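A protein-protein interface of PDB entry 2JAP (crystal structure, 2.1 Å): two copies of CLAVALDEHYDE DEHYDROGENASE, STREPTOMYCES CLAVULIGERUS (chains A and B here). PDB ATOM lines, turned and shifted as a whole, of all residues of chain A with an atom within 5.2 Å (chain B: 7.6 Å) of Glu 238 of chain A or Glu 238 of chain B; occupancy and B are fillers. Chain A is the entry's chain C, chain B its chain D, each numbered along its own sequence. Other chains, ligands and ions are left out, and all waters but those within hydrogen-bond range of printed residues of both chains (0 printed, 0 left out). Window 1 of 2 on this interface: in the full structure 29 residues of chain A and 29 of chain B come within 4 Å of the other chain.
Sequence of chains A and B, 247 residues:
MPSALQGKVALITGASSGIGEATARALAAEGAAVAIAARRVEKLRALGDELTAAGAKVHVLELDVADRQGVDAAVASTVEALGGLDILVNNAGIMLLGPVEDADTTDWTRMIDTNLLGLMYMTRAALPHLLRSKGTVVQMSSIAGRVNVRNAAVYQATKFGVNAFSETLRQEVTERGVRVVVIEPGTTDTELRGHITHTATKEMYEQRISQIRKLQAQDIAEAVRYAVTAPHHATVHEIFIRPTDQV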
ATOM      1  N   ARG A 146      28.195  16.156   2.895  1.00  0.00           N
ATOM      2  CA  ARG A 146      29.093  16.201   1.721  1.00  0.00           C
ATOM      3  C   ARG A 146      29.311  17.619   1.200  1.00  0.00           C
ATOM      4  O   ARG A 146      30.342  17.920   0.604  1.00  0.00           O
ATOM      5  CB  ARG A 146      28.550  15.348   0.566  1.00  0.00           C
ATOM      6  CG  ARG A 146      28.394  13.865   0.863  1.00  0.00           C
ATOM      7  CD  ARG A 146      29.757  13.195   1.103  1.00  0.00           C
ATOM      8  NE  ARG A 146      30.647  13.435  -0.031  1.00  0.00           N
ATOM      9  CZ  ARG A 146      30.666  12.704  -1.139  1.00  0.00           C
ATOM     10  NH1 ARG A 146      29.854  11.653  -1.269  1.00  0.00           N
ATOM     11  NH2 ARG A 146      31.494  13.027  -2.115  1.00  0.00           N
ATOM     12  N   ASN A 163      29.655  10.986   9.009  1.00  0.00           N
ATOM     13  CA  ASN A 163      30.465  10.371   7.949  1.00  0.00           C
ATOM     14  C   ASN A 163      31.874   9.983   8.402  1.00  0.00           C
ATOM     15  O   ASN A 163      32.350   8.898   8.069  1.00  0.00           O
ATOM     16  CB  ASN A 163      30.528  11.279   6.716  1.00  0.00           C
ATOM     17  CG  ASN A 163      29.194  11.353   5.992  1.00  0.00           C
ATOM     18  OD1 ASN A 163      28.178  10.870   6.484  1.00  0.00           O
ATOM     19  ND2 ASN A 163      29.198  11.954   4.826  1.00  0.00           N
ATOM     20  N   VAL A 182      26.768   4.190   4.268  1.00  0.00           N
ATOM     21  CA  VAL A 182      26.344   5.563   4.525  1.00  0.00           C
ATOM     22  C   VAL A 182      25.500   6.073   3.371  1.00  0.00           C
ATOM     23  O   VAL A 182      25.967   6.148   2.229  1.00  0.00           O
ATOM     24  CB  VAL A 182      27.537   6.522   4.758  1.00  0.00           C
ATOM     25  CG1 VAL A 182      27.025   7.921   5.068  1.00  0.00           C
ATOM     26  CG2 VAL A 182      28.461   6.000   5.901  1.00  0.00           C
ATOM     27  N   GLU A 184      23.337   9.105   1.700  1.00  0.00           N
ATOM     28  CA  GLU A 184      23.375  10.562   1.676  1.00  0.00           C
ATOM     29  C   GLU A 184      22.326  11.125   0.714  1.00  0.00           C
ATOM     30  O   GLU A 184      22.621  11.403  -0.452  1.00  0.00           O
ATOM     31  CB  GLU A 184      24.771  11.035   1.282  1.00  0.00           C
ATOM     32  CG  GLU A 184      25.822  10.726   2.322  1.00  0.00           C
ATOM     33  CD  GLU A 184      27.222  10.603   1.739  1.00  0.00           C
ATOM     34  OE1 GLU A 184      27.397  10.666   0.494  1.00  0.00           O
ATOM     35  OE2 GLU A 184      28.155  10.412   2.541  1.00  0.00           O
ATOM     36  N   VAL A 236      28.817  -1.310   0.207  1.00  0.00           N
ATOM     37  CA  VAL A 236      28.426  -0.083  -0.481  1.00  0.00           C
ATOM     38  C   VAL A 236      28.528   1.025   0.560  1.00  0.00           C
ATOM     39  O   VAL A 236      27.568   1.339   1.261  1.00  0.00           O
ATOM     40  CB  VAL A 236      27.013  -0.179  -1.119  1.00  0.00           C
ATOM     41  CG1 VAL A 236      26.702   1.097  -1.890  1.00  0.00           C
ATOM     42  CG2 VAL A 236      26.925  -1.390  -2.053  1.00  0.00           C
ATOM     43  N   HIS A 237      29.725   1.581   0.683  1.00  0.00           N
ATOM     44  CA  HIS A 237      30.011   2.491   1.776  1.00  0.00           C
ATOM     45  C   HIS A 237      29.311   3.848   1.652  1.00  0.00           C
ATOM     46  O   HIS A 237      29.002   4.471   2.667  1.00  0.00           O
ATOM     47  CB  HIS A 237      31.519   2.677   1.988  1.00  0.00           C
ATOM     48  CG  HIS A 237      31.843   3.503   3.192  1.00  0.00           C
ATOM     49  ND1 HIS A 237      31.488   3.118   4.466  1.00  0.00           N
ATOM     50  CD2 HIS A 237      32.433   4.715   3.318  1.00  0.00           C
ATOM     51  CE1 HIS A 237      31.872   4.043   5.329  1.00  0.00           C
ATOM     52  NE2 HIS A 237      32.440   5.028   4.658  1.00  0.00           N
ATOM     53  N   GLU A 238      29.087   4.303   0.424  1.00  0.00           N
ATOM     54  CA  GLU A 238      28.457   5.594   0.203  1.00  0.00           C
ATOM     55  C   GLU A 238      27.529   5.556  -0.984  1.00  0.00           C
ATOM     56  O   GLU A 238      27.912   5.117  -2.069  1.00  0.00           O
ATOM     57  CB  GLU A 238      29.501   6.705  -0.008  1.00  0.00           C
ATOM     58  CG  GLU A 238      29.613   7.684   1.136  1.00  0.00           C
ATOM     59  CD  GLU A 238      30.703   8.776   0.947  1.00  0.00           C
ATOM     60  OE1 GLU A 238      31.690   8.541   0.244  1.00  0.00           O
ATOM     61  OE2 GLU A 238      30.577   9.866   1.549  1.00  0.00           O
ATOM     62  N   ILE A 239      26.297   5.995  -0.764  1.00  0.00           N
ATOM     63  CA  ILE A 239      25.392   6.268  -1.869  1.00  0.00           C
ATOM     64  C   ILE A 239      24.954   7.704  -1.692  1.00  0.00           C
ATOM     65  O   ILE A 239      24.363   8.051  -0.670  1.00  0.00           O
ATOM     66  CB  ILE A 239      24.177   5.327  -1.899  1.00  0.00           C
ATOM     67  CG1 ILE A 239      24.612   3.851  -1.915  1.00  0.00           C
ATOM     68  CG2 ILE A 239      23.297   5.667  -3.109  1.00  0.00           C
ATOM     69  CD1 ILE A 239      23.435   2.840  -1.841  1.00  0.00           C
ATOM     70  N   PHE A 240      25.310   8.529  -2.672  1.00  0.00           N
ATOM     71  CA  PHE A 240      25.006   9.956  -2.666  1.00  0.00           C
ATOM     72  C   PHE A 240      23.945  10.158  -3.734  1.00  0.00           C
ATOM     73  O   PHE A 240      24.216  10.041  -4.923  1.00  0.00           O
ATOM     74  CB  PHE A 240      26.289  10.765  -2.944  1.00  0.00           C
ATOM     75  CG  PHE A 240      26.137  12.264  -2.796  1.00  0.00           C
ATOM     76  CD1 PHE A 240      25.037  12.824  -2.158  1.00  0.00           C
ATOM     77  CD2 PHE A 240      27.117  13.113  -3.306  1.00  0.00           C
ATOM     78  CE1 PHE A 240      24.905  14.213  -2.028  1.00  0.00           C
ATOM     79  CE2 PHE A 240      27.009  14.497  -3.177  1.00  0.00           C
ATOM     80  CZ  PHE A 240      25.899  15.056  -2.536  1.00  0.00           C
ATOM     81  N   SER B 141      34.543   5.774 -12.332  1.00  0.00           N
ATOM     82  CA  SER B 141      35.661   6.312 -11.570  1.00  0.00           C
ATOM     83  C   SER B 141      36.267   5.165 -10.770  1.00  0.00           C
ATOM     84  O   SER B 141      36.354   4.044 -11.272  1.00  0.00           O
ATOM     85  CB  SER B 141      35.193   7.449 -10.665  1.00  0.00           C
ATOM     86  OG  SER B 141      36.291   8.121 -10.078  1.00  0.00           O
ATOM     87  N   SER B 142      36.659   5.439  -9.526  1.00  0.00           N
ATOM     88  CA  SER B 142      37.355   4.469  -8.707  1.00  0.00           C
ATOM     89  C   SER B 142      37.461   4.982  -7.286  1.00  0.00           C
ATOM     90  O   SER B 142      37.246   6.179  -7.031  1.00  0.00           O
ATOM     91  CB  SER B 142      38.761   4.229  -9.270  1.00  0.00           C
ATOM     92  OG  SER B 142      39.538   3.396  -8.421  1.00  0.00           O
ATOM     93  N   GLY B 145      39.576   7.819  -7.128  1.00  0.00           N
ATOM     94  CA  GLY B 145      39.029   9.171  -7.225  1.00  0.00           C
ATOM     95  C   GLY B 145      38.552   9.728  -5.888  1.00  0.00           C
ATOM     96  O   GLY B 145      38.018  10.833  -5.833  1.00  0.00           O
ATOM     97  N   ARG B 146      38.725   8.952  -4.818  1.00  0.00           N
ATOM     98  CA  ARG B 146      38.274   9.346  -3.489  1.00  0.00           C
ATOM     99  C   ARG B 146      39.397   9.297  -2.438  1.00  0.00           C
ATOM    100  O   ARG B 146      39.364  10.034  -1.457  1.00  0.00           O
ATOM    101  CB  ARG B 146      37.084   8.474  -3.034  1.00  0.00           C
ATOM    102  CG  ARG B 146      35.835   8.538  -3.926  1.00  0.00           C
ATOM    103  CD  ARG B 146      35.113   9.919  -3.881  1.00  0.00           C
ATOM    104  NE  ARG B 146      34.793  10.333  -2.512  1.00  0.00           N
ATOM    105  CZ  ARG B 146      33.757   9.883  -1.808  1.00  0.00           C
ATOM    106  NH1 ARG B 146      32.907   9.018  -2.342  1.00  0.00           N
ATOM    107  NH2 ARG B 146      33.564  10.301  -0.570  1.00  0.00           N
ATOM    108  N   ASN B 163      36.037  12.844 -11.405  1.00  0.00           N
ATOM    109  CA  ASN B 163      35.026  13.229 -10.428  1.00  0.00           C
ATOM    110  C   ASN B 163      34.688  14.716 -10.452  1.00  0.00           C
ATOM    111  O   ASN B 163      33.515  15.082 -10.410  1.00  0.00           O
ATOM    112  CB  ASN B 163      35.430  12.790  -9.012  1.00  0.00           C
ATOM    113  CG  ASN B 163      35.278  11.298  -8.807  1.00  0.00           C
ATOM    114  OD1 ASN B 163      35.303  10.514  -9.761  1.00  0.00           O
ATOM    115  ND2 ASN B 163      35.103  10.896  -7.567  1.00  0.00           N
ATOM    116  N   GLU B 167      31.096  16.210 -11.476  1.00  0.00           N
ATOM    117  CA  GLU B 167      30.322  17.088 -10.596  1.00  0.00           C
ATOM    118  C   GLU B 167      30.013  18.407 -11.297  1.00  0.00           C
ATOM    119  O   GLU B 167      28.885  18.897 -11.251  1.00  0.00           O
ATOM    120  CB  GLU B 167      31.052  17.346  -9.264  1.00  0.00           C
ATOM    121  CG  GLU B 167      30.523  18.544  -8.440  1.00  0.00           C
ATOM    122  CD  GLU B 167      29.008  18.521  -8.183  1.00  0.00           C
ATOM    123  OE1 GLU B 167      28.375  17.439  -8.244  1.00  0.00           O
ATOM    124  OE2 GLU B 167      28.452  19.600  -7.906  1.00  0.00           O
ATOM    125  N   VAL B 180      23.932  12.653 -14.022  1.00  0.00           N
ATOM    126  CA  VAL B 180      25.345  12.308 -13.952  1.00  0.00           C
ATOM    127  C   VAL B 180      25.601  11.384 -12.764  1.00  0.00           C
ATOM    128  O   VAL B 180      25.425  11.768 -11.598  1.00  0.00           O
ATOM    129  CB  VAL B 180      26.242  13.560 -13.874  1.00  0.00           C
ATOM    130  CG1 VAL B 180      27.720  13.159 -13.804  1.00  0.00           C
ATOM    131  CG2 VAL B 180      25.982  14.460 -15.090  1.00  0.00           C
ATOM    132  N   VAL B 181      26.043  10.177 -13.094  1.00  0.00           N
ATOM    133  CA  VAL B 181      26.274   9.098 -12.143  1.00  0.00           C
ATOM    134  C   VAL B 181      27.765   8.770 -12.128  1.00  0.00           C
ATOM    135  O   VAL B 181      28.384   8.588 -13.190  1.00  0.00           O
ATOM    136  CB  VAL B 181      25.484   7.840 -12.559  1.00  0.00           C
ATOM    137  CG1 VAL B 181      25.825   6.636 -11.652  1.00  0.00           C
ATOM    138  CG2 VAL B 181      24.007   8.125 -12.530  1.00  0.00           C
ATOM    139  N   VAL B 182      28.347   8.723 -10.936  1.00  0.00           N
ATOM    140  CA  VAL B 182      29.752   8.345 -10.794  1.00  0.00           C
ATOM    141  C   VAL B 182      29.876   7.073  -9.966  1.00  0.00           C
ATOM    142  O   VAL B 182      29.467   7.031  -8.802  1.00  0.00           O
ATOM    143  CB  VAL B 182      30.623   9.464 -10.158  1.00  0.00           C
ATOM    144  CG1 VAL B 182      32.067   9.085 -10.238  1.00  0.00           C
ATOM    145  CG2 VAL B 182      30.392  10.799 -10.868  1.00  0.00           C
ATOM    146  N   ILE B 183      30.433   6.035 -10.579  1.00  0.00           N
ATOM    147  CA  ILE B 183      30.623   4.779  -9.873  1.00  0.00           C
ATOM    148  C   ILE B 183      32.074   4.704  -9.418  1.00  0.00           C
ATOM    149  O   ILE B 183      32.987   4.984 -10.189  1.00  0.00           O
ATOM    150  CB  ILE B 183      30.260   3.539 -10.746  1.00  0.00           C
ATOM    151  CG1 ILE B 183      28.902   3.741 -11.449  1.00  0.00           C
ATOM    152  CG2 ILE B 183      30.317   2.265  -9.895  1.00  0.00           C
ATOM    153  CD1 ILE B 183      27.659   3.595 -10.523  1.00  0.00           C
ATOM    154  N   GLU B 184      32.269   4.348  -8.153  1.00  0.00           N
ATOM    155  CA  GLU B 184      33.608   4.315  -7.543  1.00  0.00           C
ATOM    156  C   GLU B 184      33.875   2.951  -6.929  1.00  0.00           C
ATOM    157  O   GLU B 184      33.630   2.761  -5.741  1.00  0.00           O
ATOM    158  CB  GLU B 184      33.727   5.416  -6.474  1.00  0.00           C
ATOM    159  CG  GLU B 184      33.731   6.815  -7.073  1.00  0.00           C
ATOM    160  CD  GLU B 184      33.171   7.887  -6.142  1.00  0.00           C
ATOM    161  OE1 GLU B 184      32.741   7.587  -5.006  1.00  0.00           O
ATOM    162  OE2 GLU B 184      33.162   9.047  -6.569  1.00  0.00           O
ATOM    163  N   TYR B 226      21.366  -0.350 -10.781  1.00  0.00           N
ATOM    164  CA  TYR B 226      20.626   0.361  -9.733  1.00  0.00           C
ATOM    165  C   TYR B 226      20.526   1.872 -10.046  1.00  0.00           C
ATOM    166  O   TYR B 226      19.440   2.453  -9.986  1.00  0.00           O
ATOM    167  CB  TYR B 226      21.216   0.092  -8.323  1.00  0.00           C
ATOM    168  CG  TYR B 226      20.825   1.178  -7.331  1.00  0.00           C
ATOM    169  CD1 TYR B 226      19.502   1.302  -6.885  1.00  0.00           C
ATOM    170  CD2 TYR B 226      21.757   2.103  -6.881  1.00  0.00           C
ATOM    171  CE1 TYR B 226      19.123   2.312  -6.025  1.00  0.00           C
ATOM    172  CE2 TYR B 226      21.386   3.127  -6.002  1.00  0.00           C
ATOM    173  CZ  TYR B 226      20.069   3.223  -5.593  1.00  0.00           C
ATOM    174  OH  TYR B 226      19.697   4.231  -4.737  1.00  0.00           O
ATOM    175  N   ALA B 227      21.652   2.487 -10.401  1.00  0.00           N
ATOM    176  CA  ALA B 227      21.694   3.924 -10.671  1.00  0.00           C
ATOM    177  C   ALA B 227      20.847   4.353 -11.861  1.00  0.00           C
ATOM    178  O   ALA B 227      20.143   5.348 -11.777  1.00  0.00           O
ATOM    179  CB  ALA B 227      23.124   4.396 -10.860  1.00  0.00           C
ATOM    180  N   THR B 235      19.042  11.449  -9.049  1.00  0.00           N
ATOM    181  CA  THR B 235      20.357  11.204  -9.596  1.00  0.00           C
ATOM    182  C   THR B 235      21.242  10.564  -8.526  1.00  0.00           C
ATOM    183  O   THR B 235      21.596  11.204  -7.534  1.00  0.00           O
ATOM    184  CB  THR B 235      21.024  12.480 -10.129  1.00  0.00           C
ATOM    185  OG1 THR B 235      20.262  12.976 -11.224  1.00  0.00           O
ATOM    186  CG2 THR B 235      22.460  12.176 -10.624  1.00  0.00           C
ATOM    187  N   VAL B 236      21.577   9.294  -8.727  1.00  0.00           N
ATOM    188  CA  VAL B 236      22.512   8.610  -7.835  1.00  0.00           C
ATOM    189  C   VAL B 236      23.900   9.066  -8.266  1.00  0.00           C
ATOM    190  O   VAL B 236      24.558   8.420  -9.090  1.00  0.00           O
ATOM    191  CB  VAL B 236      22.377   7.058  -7.887  1.00  0.00           C
ATOM    192  CG1 VAL B 236      23.306   6.394  -6.876  1.00  0.00           C
ATOM    193  CG2 VAL B 236      20.949   6.619  -7.618  1.00  0.00           C
ATOM    194  N   HIS B 237      24.324  10.204  -7.727  1.00  0.00           N
ATOM    195  CA  HIS B 237      25.517  10.853  -8.215  1.00  0.00           C
ATOM    196  C   HIS B 237      26.801  10.089  -7.886  1.00  0.00           C
ATOM    197  O   HIS B 237      27.743  10.119  -8.663  1.00  0.00           O
ATOM    198  CB  HIS B 237      25.604  12.303  -7.746  1.00  0.00           C
ATOM    199  CG  HIS B 237      26.795  13.022  -8.298  1.00  0.00           C
ATOM    200  ND1 HIS B 237      26.990  13.199  -9.649  1.00  0.00           N
ATOM    201  CD2 HIS B 237      27.877  13.557  -7.689  1.00  0.00           C
ATOM    202  CE1 HIS B 237      28.130  13.836  -9.849  1.00  0.00           C
ATOM    203  NE2 HIS B 237      28.695  14.053  -8.674  1.00  0.00           N
ATOM    204  N   GLU B 238      26.826   9.398  -6.748  1.00  0.00           N
ATOM    205  CA  GLU B 238      28.009   8.624  -6.355  1.00  0.00           C
ATOM    206  C   GLU B 238      27.607   7.345  -5.673  1.00  0.00           C
ATOM    207  O   GLU B 238      26.784   7.356  -4.757  1.00  0.00           O
ATOM    208  CB  GLU B 238      28.923   9.396  -5.398  1.00  0.00           C
ATOM    209  CG  GLU B 238      30.009  10.201  -6.059  1.00  0.00           C
ATOM    210  CD  GLU B 238      30.863  10.973  -5.059  1.00  0.00           C
ATOM    211  OE1 GLU B 238      30.308  11.733  -4.236  1.00  0.00           O
ATOM    212  OE2 GLU B 238      32.094  10.839  -5.113  1.00  0.00           O
ATOM    213  N   ILE B 239      28.201   6.250  -6.129  1.00  0.00           N
ATOM    214  CA  ILE B 239      28.169   4.985  -5.396  1.00  0.00           C
ATOM    215  C   ILE B 239      29.609   4.578  -5.170  1.00  0.00           C
ATOM    216  O   ILE B 239      30.369   4.359  -6.119  1.00  0.00           O
ATOM    217  CB  ILE B 239      27.436   3.866  -6.160  1.00  0.00           C
ATOM    218  CG1 ILE B 239      26.049   4.343  -6.609  1.00  0.00           C
ATOM    219  CG2 ILE B 239      27.321   2.601  -5.279  1.00  0.00           C
ATOM    220  CD1 ILE B 239      25.257   3.327  -7.440  1.00  0.00           C
ATOM    221  N   PHE B 240      29.977   4.485  -3.906  1.00  0.00           N
ATOM    222  CA  PHE B 240      31.339   4.156  -3.523  1.00  0.00           C
ATOM    223  C   PHE B 240      31.242   2.771  -2.934  1.00  0.00           C
ATOM    224  O   PHE B 240      30.726   2.585  -1.838  1.00  0.00           O
ATOM    225  CB  PHE B 240      31.855   5.201  -2.518  1.00  0.00           C
ATOM    226  CG  PHE B 240      33.304   5.031  -2.103  1.00  0.00           C
ATOM    227  CD1 PHE B 240      34.180   4.188  -2.797  1.00  0.00           C
ATOM    228  CD2 PHE B 240      33.798   5.763  -1.030  1.00  0.00           C
ATOM    229  CE1 PHE B 240      35.505   4.052  -2.409  1.00  0.00           C
ATOM    230  CE2 PHE B 240      35.135   5.649  -0.637  1.00  0.00           C
ATOM    231  CZ  PHE B 240      35.992   4.796  -1.317  1.00  0.00           C
ATOM    232  N   ILE B 241      31.712   1.788  -3.698  1.00  0.00           N
ATOM    233  CA  ILE B 241      31.615   0.397  -3.291  1.00  0.00           C
ATOM    234  C   ILE B 241      33.008  -0.211  -3.072  1.00  0.00           C
ATOM    235  O   ILE B 241      33.863  -0.191  -3.968  1.00  0.00           O
ATOM    236  CB  ILE B 241      30.697  -0.425  -4.269  1.00  0.00           C
ATOM    237  CG1 ILE B 241      30.715  -1.919  -3.927  1.00  0.00           C
ATOM    238  CG2 ILE B 241      31.038  -0.142  -5.734  1.00  0.00           C
ATOM    239  CD1 ILE B 241      29.634  -2.734  -4.701  1.00  0.00           C
ATOM    240  N   ARG B 242      33.219  -0.728  -1.867  1.00  0.00           N
ATOM    241  CA  ARG B 242      34.528  -1.219  -1.426  1.00  0.00           C
ATOM    242  C   ARG B 242      34.447  -2.704  -1.108  1.00  0.00           C
ATOM    243  O   ARG B 242      33.380  -3.208  -0.730  1.00  0.00           O
ATOM    244  CB  ARG B 242      34.958  -0.540  -0.132  1.00  0.00           C
ATOM    245  CG  ARG B 242      35.307   0.901  -0.201  1.00  0.00           C
ATOM    246  CD  ARG B 242      35.502   1.328   1.234  1.00  0.00           C
ATOM    247  NE  ARG B 242      36.064   2.655   1.392  1.00  0.00           N
ATOM    248  CZ  ARG B 242      37.356   2.915   1.547  1.00  0.00           C
ATOM    249  NH1 ARG B 242      38.253   1.938   1.543  1.00  0.00           N
ATOM    250  NH2 ARG B 242      37.744   4.168   1.703  1.00  0.00           N
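OE1 of Glu 238 of chain B is in salt-bridge range of NH2 of Arg 146 of chain A, 2.8 Å away.
N of His 237 of chain A sits at hydrogen-bond distance from O of Phe 240 of chain B (2.9 Å).
OE1 of Glu 238 of chain A is in salt-bridge range of NH2 of Arg 146 of chain B, 2.7 Å away.
The backbone carbonyl oxygen (O) of Glu 238 of chain A sits at hydrogen-bond distance from the backbone NH (N) of Phe 240 of chain B.
N of His 237 of chain B sits at hydrogen-bond distance from O of Phe 240 of chain A (2.8 Å).
The backbone NH (N) of Phe 240 of chain A is in hydrogen-bond range of the backbone carbonyl oxygen (O) of Glu 238 of chain B, 2.8 Å away.
The backbone carbonyl oxygen (O) of Val 182 of chain A sits at hydrogen-bond distance from the backbone NH (N) of Ile 239 of chain A (3.0 Å).
OE2 of Glu 238 of chain A lies close to OE2 of Glu 184 of chain A.
NH1 of Arg 146 of chain B is in salt-bridge range of OE1 of Glu 184 of chain B, 3.0 Å away.
OE1 of Glu 167 of chain B lies within hydrogen-bond range of NE2 of His 237 of chain B (3.4 Å).
OE2 of Glu 184 of chain B lies close to OE2 of Glu 238 of chain B (2.5 Å).
N of Glu 184 of chain B lies within hydrogen-bond range of O of Ile 239 of chain B (2.8 Å).
Among the printed residues, pairs that only touch across the chains: Arg 146 of chain A with Arg 146 of chain B (3.8 Å), Val 236 of chain A with Ile 239 of chain B (3.8 Å), Val 236 of chain A with Phe 240 of chain B (3.6 Å), Glu 238 of chain A with Glu 238 of chain B (3.7 Å), Glu 238 of chain A with Ile 239 of chain B (3.3 Å), Ile 239 of chain A with Val 236 of chain B (3.8 Å), Ile 239 of chain A with Glu 238 of chain B (3.4 Å), Phe 240 of chain A with Thr 235 of chain B (3.9 Å) and Phe 240 of chain A with Val 236 of chain B (3.5 Å).
Glu 238 of chain A touches just these residues of chain B: Arg 146, Glu 238, Ile 239 and Phe 240.
Of chain A, only Arg 146 (2.8 Å), Glu 238 (3.7 Å), Ile 239 (3.4 Å) and Phe 240 (2.8 Å) come within 4 Å of Glu 238 of chain B.
Of the printed residues of chain B, Val 236 of chain A touches Ile 239 (3.8 Å) and Phe 240 (3.6 Å).
Of the printed residues of chain A, Val 236 of chain B touches Ile 239 and Phe 240.
Of the printed residues of chain A, Arg 146 of chain B touches Arg 146 and Glu 238.
Of the printed residues of chain A, His 237 of chain B touches Phe 240 (2.8 Å).
The nearest residue of chain B that does not touch Glu 238 of chain A is Ile 241 of chain B (5.3 Å).
The nearest printed residue of chain A that does not touch Glu 238 of chain B is Glu 184 of chain A (5.7 Å).
The nearest printed residue of chain A that does not touch Ile 239 of chain B is Ile 239 of chain A (4.5 Å).
Of the 21 printed residues of chain B, 7 touch a printed residue of chain A.
Printed residues of chain A that touch a printed residue of chain B: Arg 146, Val 236, His 237, Glu 238, Ile 239 and Phe 240.
Hydrophobic or aromatic side chains of chain A that line the printed part of chain B: Val 236, His 237, Ile 239 and Phe 240.
Along chain A the printed residues that touch a printed residue of chain B span positions 146 to 240.
Among the printed residues, 15 pairs touch across the chains.
Arg 146 of chain A touches its own counterpart, Arg 146 of chain B.
Val 236 of chain A touches Phe 240 of chain B, and with the chains exchanged Phe 240 of chain A touches Val 236 of chain B.
His 237 of chain A touches Phe 240 of chain B, and with the chains exchanged Phe 240 of chain A touches His 237 of chain B.
Glu 238 of chain A touches Ile 239 of chain B, and with the chains exchanged Ile 239 of chain A touches Glu 238 of chain B.
Of the 15 pairs that touch across the chains among the printed residues, 14 have their exchanged pair printed and touching as well.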
